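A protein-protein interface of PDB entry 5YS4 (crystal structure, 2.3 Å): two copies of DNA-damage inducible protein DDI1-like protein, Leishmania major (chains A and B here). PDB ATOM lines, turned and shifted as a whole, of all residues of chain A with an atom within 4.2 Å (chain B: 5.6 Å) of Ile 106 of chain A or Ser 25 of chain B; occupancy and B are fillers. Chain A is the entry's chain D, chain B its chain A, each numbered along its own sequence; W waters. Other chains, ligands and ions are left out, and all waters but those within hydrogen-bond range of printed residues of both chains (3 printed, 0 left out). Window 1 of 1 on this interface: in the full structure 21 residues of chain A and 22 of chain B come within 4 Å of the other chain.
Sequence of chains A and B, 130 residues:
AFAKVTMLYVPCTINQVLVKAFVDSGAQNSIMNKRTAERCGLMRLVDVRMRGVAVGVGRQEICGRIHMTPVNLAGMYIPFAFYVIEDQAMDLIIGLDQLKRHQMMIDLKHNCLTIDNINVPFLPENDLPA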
ATOM      1  N   MET A   7      24.162  11.148   0.364  1.00  0.00           N
ATOM      2  CA  MET A   7      23.310  11.994  -0.456  1.00  0.00           C
ATOM      3  C   MET A   7      22.705  13.118   0.383  1.00  0.00           C
ATOM      4  O   MET A   7      22.615  13.035   1.611  1.00  0.00           O
ATOM      5  CB  MET A   7      22.211  11.165  -1.122  1.00  0.00           C
ATOM      6  CG  MET A   7      22.744  10.017  -1.973  1.00  0.00           C
ATOM      7  SD  MET A   7      23.725  10.474  -3.428  1.00  0.00           S
ATOM      8  CE  MET A   7      22.943  11.994  -3.965  1.00  0.00           C
ATOM      9  N   LEU A   8      22.287  14.180  -0.300  1.00  0.00           N
ATOM     10  CA  LEU A   8      21.867  15.407   0.367  1.00  0.00           C
ATOM     11  C   LEU A   8      20.409  15.315   0.801  1.00  0.00           C
ATOM     12  O   LEU A   8      19.513  15.152  -0.035  1.00  0.00           O
ATOM     13  CB  LEU A   8      22.071  16.605  -0.555  1.00  0.00           C
ATOM     14  CG  LEU A   8      23.497  16.819  -1.060  1.00  0.00           C
ATOM     15  CD1 LEU A   8      23.579  18.091  -1.887  1.00  0.00           C
ATOM     16  CD2 LEU A   8      24.474  16.856   0.104  1.00  0.00           C
ATOM     17  N   VAL A  23      17.547  16.823  -1.909  1.00  0.00           N
ATOM     18  CA  VAL A  23      18.014  18.013  -2.615  1.00  0.00           C
ATOM     19  C   VAL A  23      18.686  17.550  -3.902  1.00  0.00           C
ATOM     20  O   VAL A  23      19.743  16.910  -3.866  1.00  0.00           O
ATOM     21  CB  VAL A  23      18.969  18.848  -1.755  1.00  0.00           C
ATOM     22  CG1 VAL A  23      19.516  20.022  -2.560  1.00  0.00           C
ATOM     23  CG2 VAL A  23      18.259  19.335  -0.505  1.00  0.00           C
ATOM     24  N   ASP A  24      18.079  17.882  -5.040  1.00  0.00           N
ATOM     25  CA  ASP A  24      18.529  17.400  -6.345  1.00  0.00           C
ATOM     26  C   ASP A  24      18.591  18.582  -7.308  1.00  0.00           C
ATOM     27  O   ASP A  24      17.562  19.019  -7.831  1.00  0.00           O
ATOM     28  CB  ASP A  24      17.591  16.309  -6.857  1.00  0.00           C
ATOM     29  CG  ASP A  24      18.127  15.600  -8.087  1.00  0.00           C
ATOM     30  OD1 ASP A  24      19.090  16.098  -8.704  1.00  0.00           O
ATOM     31  OD2 ASP A  24      17.573  14.536  -8.439  1.00  0.00           O
ATOM     32  N   SER A  25      19.803  19.091  -7.546  1.00  0.00           N
ATOM     33  CA  SER A  25      19.992  20.163  -8.517  1.00  0.00           C
ATOM     34  C   SER A  25      19.790  19.683  -9.949  1.00  0.00           C
ATOM     35  O   SER A  25      19.574  20.507 -10.843  1.00  0.00           O
ATOM     36  CB  SER A  25      21.385  20.778  -8.368  1.00  0.00           C
ATOM     37  OG  SER A  25      22.391  19.895  -8.838  1.00  0.00           O
ATOM     38  N   MET A 105      21.230  27.934  -1.824  1.00  0.00           N
ATOM     39  CA  MET A 105      22.643  27.664  -2.050  1.00  0.00           C
ATOM     40  C   MET A 105      22.974  26.296  -1.484  1.00  0.00           C
ATOM     41  O   MET A 105      22.783  26.057  -0.287  1.00  0.00           O
ATOM     42  CB  MET A 105      23.497  28.742  -1.384  1.00  0.00           C
ATOM     43  CG  MET A 105      23.442  30.076  -2.090  1.00  0.00           C
ATOM     44  SD  MET A 105      24.437  31.311  -1.251  1.00  0.00           S
ATOM     45  CE  MET A 105      23.908  32.790  -2.100  1.00  0.00           C
ATOM     46  N   ILE A 106      23.461  25.402  -2.339  1.00  0.00           N
ATOM     47  CA  ILE A 106      23.917  24.087  -1.907  1.00  0.00           C
ATOM     48  C   ILE A 106      25.398  24.238  -1.575  1.00  0.00           C
ATOM     49  O   ILE A 106      26.253  24.226  -2.462  1.00  0.00           O
ATOM     50  CB  ILE A 106      23.670  23.016  -2.969  1.00  0.00           C
ATOM     51  CG1 ILE A 106      22.182  22.943  -3.311  1.00  0.00           C
ATOM     52  CG2 ILE A 106      24.169  21.664  -2.488  1.00  0.00           C
ATOM     53  CD1 ILE A 106      21.889  22.177  -4.583  1.00  0.00           C
ATOM     54  N   ASP A 107      25.696  24.392  -0.289  1.00  0.00           N
ATOM     55  CA  ASP A 107      27.050  24.659   0.187  1.00  0.00           C
ATOM     56  C   ASP A 107      27.640  23.332   0.646  1.00  0.00           C
ATOM     57  O   ASP A 107      27.304  22.827   1.720  1.00  0.00           O
ATOM     58  CB  ASP A 107      27.030  25.691   1.311  1.00  0.00           C
ATOM     59  CG  ASP A 107      28.417  26.201   1.671  1.00  0.00           C
ATOM     60  OD1 ASP A 107      29.417  25.513   1.374  1.00  0.00           O
ATOM     61  OD2 ASP A 107      28.504  27.299   2.262  1.00  0.00           O
ATOM     62  N   LEU A 108      28.519  22.766  -0.176  1.00  0.00           N
ATOM     63  CA  LEU A 108      29.189  21.516   0.147  1.00  0.00           C
ATOM     64  C   LEU A 108      30.559  21.731   0.772  1.00  0.00           C
ATOM     65  O   LEU A 108      31.208  20.756   1.166  1.00  0.00           O
ATOM     66  CB  LEU A 108      29.297  20.650  -1.108  1.00  0.00           C
ATOM     67  CG  LEU A 108      27.906  20.403  -1.697  1.00  0.00           C
ATOM     68  CD1 LEU A 108      27.974  20.144  -3.187  1.00  0.00           C
ATOM     69  CD2 LEU A 108      27.213  19.253  -0.979  1.00  0.00           C
ATOM     70  N   CYS A 112      25.810  22.306   4.078  1.00  0.00           N
ATOM     71  CA  CYS A 112      24.534  22.886   4.474  1.00  0.00           C
ATOM     72  C   CYS A 112      23.839  23.469   3.253  1.00  0.00           C
ATOM     73  O   CYS A 112      24.473  23.802   2.249  1.00  0.00           O
ATOM     74  CB  CYS A 112      24.710  23.975   5.537  1.00  0.00           C
ATOM     75  SG  CYS A 112      25.545  25.464   4.935  1.00  0.00           S
ATOM     76  N   LEU A 113      22.520  23.586   3.362  1.00  0.00           N
ATOM     77  CA  LEU A 113      21.698  24.286   2.388  1.00  0.00           C
ATOM     78  C   LEU A 113      21.352  25.657   2.956  1.00  0.00           C
ATOM     79  O   LEU A 113      20.806  25.752   4.061  1.00  0.00           O
ATOM     80  CB  LEU A 113      20.430  23.494   2.070  1.00  0.00           C
ATOM     81  CG  LEU A 113      19.470  24.116   1.055  1.00  0.00           C
ATOM     82  CD1 LEU A 113      20.024  23.990  -0.358  1.00  0.00           C
ATOM     83  CD2 LEU A 113      18.095  23.480   1.159  1.00  0.00           C
ATOM     84  N   PHE A 122      22.985  19.435   6.222  1.00  0.00           N
ATOM     85  CA  PHE A 122      22.523  18.211   5.590  1.00  0.00           C
ATOM     86  C   PHE A 122      22.542  17.069   6.596  1.00  0.00           C
ATOM     87  O   PHE A 122      23.452  16.964   7.422  1.00  0.00           O
ATOM     88  CB  PHE A 122      23.389  17.878   4.376  1.00  0.00           C
ATOM     89  CG  PHE A 122      23.251  18.861   3.247  1.00  0.00           C
ATOM     90  CD1 PHE A 122      22.012  19.122   2.687  1.00  0.00           C
ATOM     91  CD2 PHE A 122      24.361  19.519   2.740  1.00  0.00           C
ATOM     92  CE1 PHE A 122      21.880  20.025   1.649  1.00  0.00           C
ATOM     93  CE2 PHE A 122      24.237  20.422   1.701  1.00  0.00           C
ATOM     94  CZ  PHE A 122      22.996  20.676   1.153  1.00  0.00           C
ATOM     95  N   VAL B  23      25.679  19.598 -13.796  1.00  0.00           N
ATOM     96  CA  VAL B  23      25.843  19.693 -12.349  1.00  0.00           C
ATOM     97  C   VAL B  23      24.617  19.063 -11.703  1.00  0.00           C
ATOM     98  O   VAL B  23      23.508  19.598 -11.802  1.00  0.00           O
ATOM     99  CB  VAL B  23      26.026  21.147 -11.897  1.00  0.00           C
ATOM    100  CG1 VAL B  23      26.101  21.223 -10.379  1.00  0.00           C
ATOM    101  CG2 VAL B  23      27.265  21.748 -12.536  1.00  0.00           C
ATOM    102  N   ASP B  24      24.815  17.932 -11.025  1.00  0.00           N
ATOM    103  CA  ASP B  24      23.718  17.151 -10.455  1.00  0.00           C
ATOM    104  C   ASP B  24      24.074  16.787  -9.015  1.00  0.00           C
ATOM    105  O   ASP B  24      24.838  15.848  -8.777  1.00  0.00           O
ATOM    106  CB  ASP B  24      23.456  15.903 -11.296  1.00  0.00           C
ATOM    107  CG  ASP B  24      22.178  15.180 -10.901  1.00  0.00           C
ATOM    108  OD1 ASP B  24      21.612  15.481  -9.831  1.00  0.00           O
ATOM    109  OD2 ASP B  24      21.740  14.297 -11.670  1.00  0.00           O
ATOM    110  N   SER B  25      23.502  17.521  -8.057  1.00  0.00           N
ATOM    111  CA  SER B  25      23.700  17.196  -6.649  1.00  0.00           C
ATOM    112  C   SER B  25      22.986  15.909  -6.253  1.00  0.00           C
ATOM    113  O   SER B  25      23.326  15.317  -5.222  1.00  0.00           O
ATOM    114  CB  SER B  25      23.221  18.350  -5.766  1.00  0.00           C
ATOM    115  OG  SER B  25      21.807  18.440  -5.764  1.00  0.00           O
ATOM    116  N   GLY B  26      22.000  15.475  -7.036  1.00  0.00           N
ATOM    117  CA  GLY B  26      21.321  14.220  -6.781  1.00  0.00           C
ATOM    118  C   GLY B  26      22.003  12.999  -7.350  1.00  0.00           C
ATOM    119  O   GLY B  26      21.547  11.879  -7.101  1.00  0.00           O
ATOM    120  N   ALA B  27      23.083  13.186  -8.107  1.00  0.00           N
ATOM    121  CA  ALA B  27      23.821  12.077  -8.693  1.00  0.00           C
ATOM    122  C   ALA B  27      24.958  11.673  -7.764  1.00  0.00           C
ATOM    123  O   ALA B  27      25.748  12.518  -7.334  1.00  0.00           O
ATOM    124  CB  ALA B  27      24.371  12.456 -10.070  1.00  0.00           C
ATOM    125  N   ILE B  94      28.757  16.030 -13.313  1.00  0.00           N
ATOM    126  CA  ILE B  94      29.491  16.307 -12.082  1.00  0.00           C
ATOM    127  C   ILE B  94      28.582  15.901 -10.926  1.00  0.00           C
ATOM    128  O   ILE B  94      27.630  16.608 -10.584  1.00  0.00           O
ATOM    129  CB  ILE B  94      29.920  17.771 -11.988  1.00  0.00           C
ATOM    130  CG1 ILE B  94      30.913  18.112 -13.102  1.00  0.00           C
ATOM    131  CG2 ILE B  94      30.541  18.059 -10.631  1.00  0.00           C
ATOM    132  CD1 ILE B  94      31.385  19.552 -13.076  1.00  0.00           C
ATOM    133  N   GLY B  95      28.873  14.744 -10.326  1.00  0.00           N
ATOM    134  CA  GLY B  95      28.054  14.213  -9.260  1.00  0.00           C
ATOM    135  C   GLY B  95      28.473  14.723  -7.894  1.00  0.00           C
ATOM    136  O   GLY B  95      29.402  15.516  -7.746  1.00  0.00           O
ATOM    137  N   LEU B  96      27.761  14.234  -6.874  1.00  0.00           N
ATOM    138  CA  LEU B  96      28.001  14.694  -5.509  1.00  0.00           C
ATOM    139  C   LEU B  96      29.395  14.321  -5.022  1.00  0.00           C
ATOM    140  O   LEU B  96      29.967  15.027  -4.184  1.00  0.00           O
ATOM    141  CB  LEU B  96      26.937  14.125  -4.571  1.00  0.00           C
ATOM    142  CG  LEU B  96      26.827  14.786  -3.197  1.00  0.00           C
ATOM    143  CD1 LEU B  96      26.611  16.284  -3.351  1.00  0.00           C
ATOM    144  CD2 LEU B  96      25.704  14.161  -2.387  1.00  0.00           C
ATOM    145  N   LEU B  99      31.560  17.109  -6.299  1.00  0.00           N
ATOM    146  CA  LEU B  99      31.107  18.374  -5.729  1.00  0.00           C
ATOM    147  C   LEU B  99      31.579  18.529  -4.289  1.00  0.00           C
ATOM    148  O   LEU B  99      32.003  19.615  -3.878  1.00  0.00           O
ATOM    149  CB  LEU B  99      29.584  18.467  -5.812  1.00  0.00           C
ATOM    150  CG  LEU B  99      28.975  18.684  -7.198  1.00  0.00           C
ATOM    151  CD1 LEU B  99      27.522  18.241  -7.211  1.00  0.00           C
ATOM    152  CD2 LEU B  99      29.100  20.141  -7.620  1.00  0.00           C
ATOM    153  N   MET B 104      32.748  22.417  -3.462  1.00  0.00           N
ATOM    154  CA  MET B 104      32.070  23.334  -4.361  1.00  0.00           C
ATOM    155  C   MET B 104      30.803  23.890  -3.714  1.00  0.00           C
ATOM    156  O   MET B 104      30.308  23.384  -2.703  1.00  0.00           O
ATOM    157  CB  MET B 104      31.730  22.638  -5.676  1.00  0.00           C
ATOM    158  CG  MET B 104      32.915  21.961  -6.342  1.00  0.00           C
ATOM    159  SD  MET B 104      32.548  21.492  -8.042  1.00  0.00           S
ATOM    160  CE  MET B 104      33.951  20.445  -8.422  1.00  0.00           C
ATOM    161  N   MET B 105      30.275  24.950  -4.322  1.00  0.00           N
ATOM    162  CA  MET B 105      29.041  25.580  -3.870  1.00  0.00           C
ATOM    163  C   MET B 105      28.176  25.856  -5.088  1.00  0.00           C
ATOM    164  O   MET B 105      28.612  26.544  -6.016  1.00  0.00           O
ATOM    165  CB  MET B 105      29.309  26.878  -3.104  1.00  0.00           C
ATOM    166  CG  MET B 105      29.849  26.685  -1.698  1.00  0.00           C
ATOM    167  SD  MET B 105      30.075  28.264  -0.859  1.00  0.00           S
ATOM    168  CE  MET B 105      31.858  28.396  -0.831  1.00  0.00           C
ATOM    169  N   ILE B 106      26.965  25.305  -5.093  1.00  0.00           N
ATOM    170  CA  ILE B 106      25.999  25.565  -6.152  1.00  0.00           C
ATOM    171  C   ILE B 106      25.188  26.779  -5.709  1.00  0.00           C
ATOM    172  O   ILE B 106      24.259  26.667  -4.906  1.00  0.00           O
ATOM    173  CB  ILE B 106      25.113  24.351  -6.426  1.00  0.00           C
ATOM    174  CG1 ILE B 106      25.977  23.145  -6.806  1.00  0.00           C
ATOM    175  CG2 ILE B 106      24.119  24.662  -7.537  1.00  0.00           C
ATOM    176  CD1 ILE B 106      25.241  21.825  -6.754  1.00  0.00           C
ATOM    177  N   ASP B 107      25.552  27.947  -6.228  1.00  0.00           N
ATOM    178  CA  ASP B 107      24.957  29.219  -5.828  1.00  0.00           C
ATOM    179  C   ASP B 107      23.902  29.592  -6.863  1.00  0.00           C
ATOM    180  O   ASP B 107      24.226  30.045  -7.962  1.00  0.00           O
ATOM    181  CB  ASP B 107      26.031  30.296  -5.705  1.00  0.00           C
ATOM    182  CG  ASP B 107      25.516  31.573  -5.061  1.00  0.00           C
ATOM    183  OD1 ASP B 107      24.289  31.812  -5.081  1.00  0.00           O
ATOM    184  OD2 ASP B 107      26.347  32.343  -4.532  1.00  0.00           O
ATOM    185  N   LEU B 108      22.632  29.412  -6.502  1.00  0.00           N
ATOM    186  CA  LEU B 108      21.531  29.765  -7.384  1.00  0.00           C
ATOM    187  C   LEU B 108      20.976  31.154  -7.115  1.00  0.00           C
ATOM    188  O   LEU B 108      20.107  31.612  -7.862  1.00  0.00           O
ATOM    189  CB  LEU B 108      20.417  28.724  -7.265  1.00  0.00           C
ATOM    190  CG  LEU B 108      20.952  27.327  -7.583  1.00  0.00           C
ATOM    191  CD1 LEU B 108      20.142  26.268  -6.884  1.00  0.00           C
ATOM    192  CD2 LEU B 108      20.972  27.092  -9.086  1.00  0.00           C
HETATM  193  O   HOH W   1      21.437  14.674  -3.110  1.00  0.00           O
HETATM  194  O   HOH W   2      21.097  20.763 -13.077  1.00  0.00           O
HETATM  195  O   HOH W   3      26.655  29.342  -1.782  1.00  0.00           O
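The backbone carbonyl oxygen of Val 23 of chain B sits at hydrogen-bond distance from the side-chain hydroxyl of Ser 25 of chain A, at 3.2 Å.
OG of Ser 25 of chain B lies within hydrogen-bond range of O of Val 23 of chain A.
N of Ser 25 of chain B lies within hydrogen-bond range of OG of Ser 25 of chain A, at 2.7 Å.
N of Gly 26 of chain B lies within hydrogen-bond range of OD1 of Asp 24 of chain A.
The backbone NH of Leu 108 of chain A lies within hydrogen-bond range of the backbone carbonyl oxygen of Met 104 of chain B (3.2 Å).
N of Ile 106 of chain B is in hydrogen-bond range of O of Ile 106 of chain A.
The side-chain carboxylate (OD1) of Asp 24 of chain A lies close to the side-chain carboxylate (OD1) of Asp 24 of chain B (2.8 Å).
SD of Met 105 of chain B sits close to OD1 of Asp 107 of chain A.
The side-chain carboxylate (OD1) of Asp 24 of chain B sits at hydrogen-bond distance from the backbone NH (N) of Gly 26 of chain B (2.8 Å).
OD1 of Asp 24 of chain B is in hydrogen-bond range of N of Ala 27 of chain B.
O of Ile 94 of chain B sits at hydrogen-bond distance from N of Asp 24 of chain B (3.1 Å).
The backbone NH of Leu 96 of chain B lies within hydrogen-bond range of the backbone carbonyl oxygen of Ala 27 of chain B (2.7 Å).
The backbone carbonyl oxygen of Leu 8 of chain A is in hydrogen-bond range of the backbone NH of Val 23 of chain A (3.2 Å).
The backbone carbonyl oxygen (O) of Asp 107 of chain A is in hydrogen-bond range of the backbone NH (N) of Cys 112 of chain A.
Among the printed residues, merely in contact across the chains: Met 7 of chain A with Ser 25 of chain B, Met 7 of chain A with Gly 26 of chain B, Met 7 of chain A with Leu 96 of chain B, Leu 8 of chain A with Ser 25 of chain B, Leu 8 of chain A with Leu 96 of chain B, Asp 24 of chain A with Ser 25 of chain B, Ser 25 of chain A with Asp 24 of chain B, Met 105 of chain A with Ile 106 of chain B, Met 105 of chain A with Asp 107 of chain B, Ile 106 of chain A with Ser 25 of chain B, Ile 106 of chain A with Met 105 of chain B, Leu 108 of chain A with Leu 96 of chain B and Leu 108 of chain A with Leu 99 of chain B.
Of chain B, only Ser 25 (3.9 Å), Met 105 (3.4 Å) and Ile 106 (2.9 Å) come within 4 Å of Ile 106 of chain A.
Of chain A, only Met 7, Leu 8, Val 23, Asp 24, Ser 25 and Ile 106 come within 4 Å of Ser 25 of chain B.
Ile 94 of chain B touches none of the printed residues of chain A.
Of the printed residues of chain A, Met 104 of chain B touches Leu 108.
Of the printed residues of chain A, Met 105 of chain B touches Ile 106 (3.4 Å) and Asp 107 (3.3 Å).
Printed residues of chain A within 4 Å of Asp 107 of chain B: Met 105 (3.2 Å).
The nearest residue of chain B that does not touch Ile 106 of chain A is Met 104 of chain B (4.1 Å).
The nearest printed residue of chain B that does not touch Leu 108 of chain A is Met 105 of chain B (4.4 Å).
Hydrophobic or aromatic side chains of chain B that line the printed part of chain A: Leu 96, Leu 99, Met 105 and Ile 106.
Printed residues of chain A that touch a printed residue of chain B: Met 7, Leu 8, Val 23, Asp 24, Ser 25, Met 105, Ile 106, Asp 107 and Leu 108.
Among the printed residues, 21 pairs touch across the chains.
Among the printed residues, no Asp or Glu carboxylate lies within 4 Å of a Lys or Arg side-chain nitrogen of the other chain.
Asp 24 of chain A touches its own counterpart, Asp 24 of chain B.
Met 105 of chain A touches Asp 107 of chain B, and with the chains exchanged Asp 107 of chain A touches Met 105 of chain B.
Ile 106 of chain A touches Ser 25 of chain B, but with the chains exchanged Ser 25 of chain A does not touch Ile 106 of chain B (4.02 Å).
Ile 106 of chain A touches its own counterpart, Ile 106 of chain B.
Of the 21 pairs that touch across the chains among the printed residues, 11 have their exchanged pair printed and touching as well.
Water W2 lies within hydrogen-bond range of O of Ser 25 of chain A (2.7 Å) and O of Val 23 of chain B (3.0 Å).
Water W1 lies within hydrogen-bond range of the backbone carbonyl oxygen of Val 23 of chain A (2.9 Å), the backbone carbonyl oxygen of Ser 25 of chain B (2.9 Å) and the backbone NH of Leu 8 of chain A (3.0 Å).
Water W3 bridges the side-chain sulfur (SD) of Met 105 of chain A (3.0 Å) and the side-chain sulfur (SD) of Met 105 of chain B (3.7 Å).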
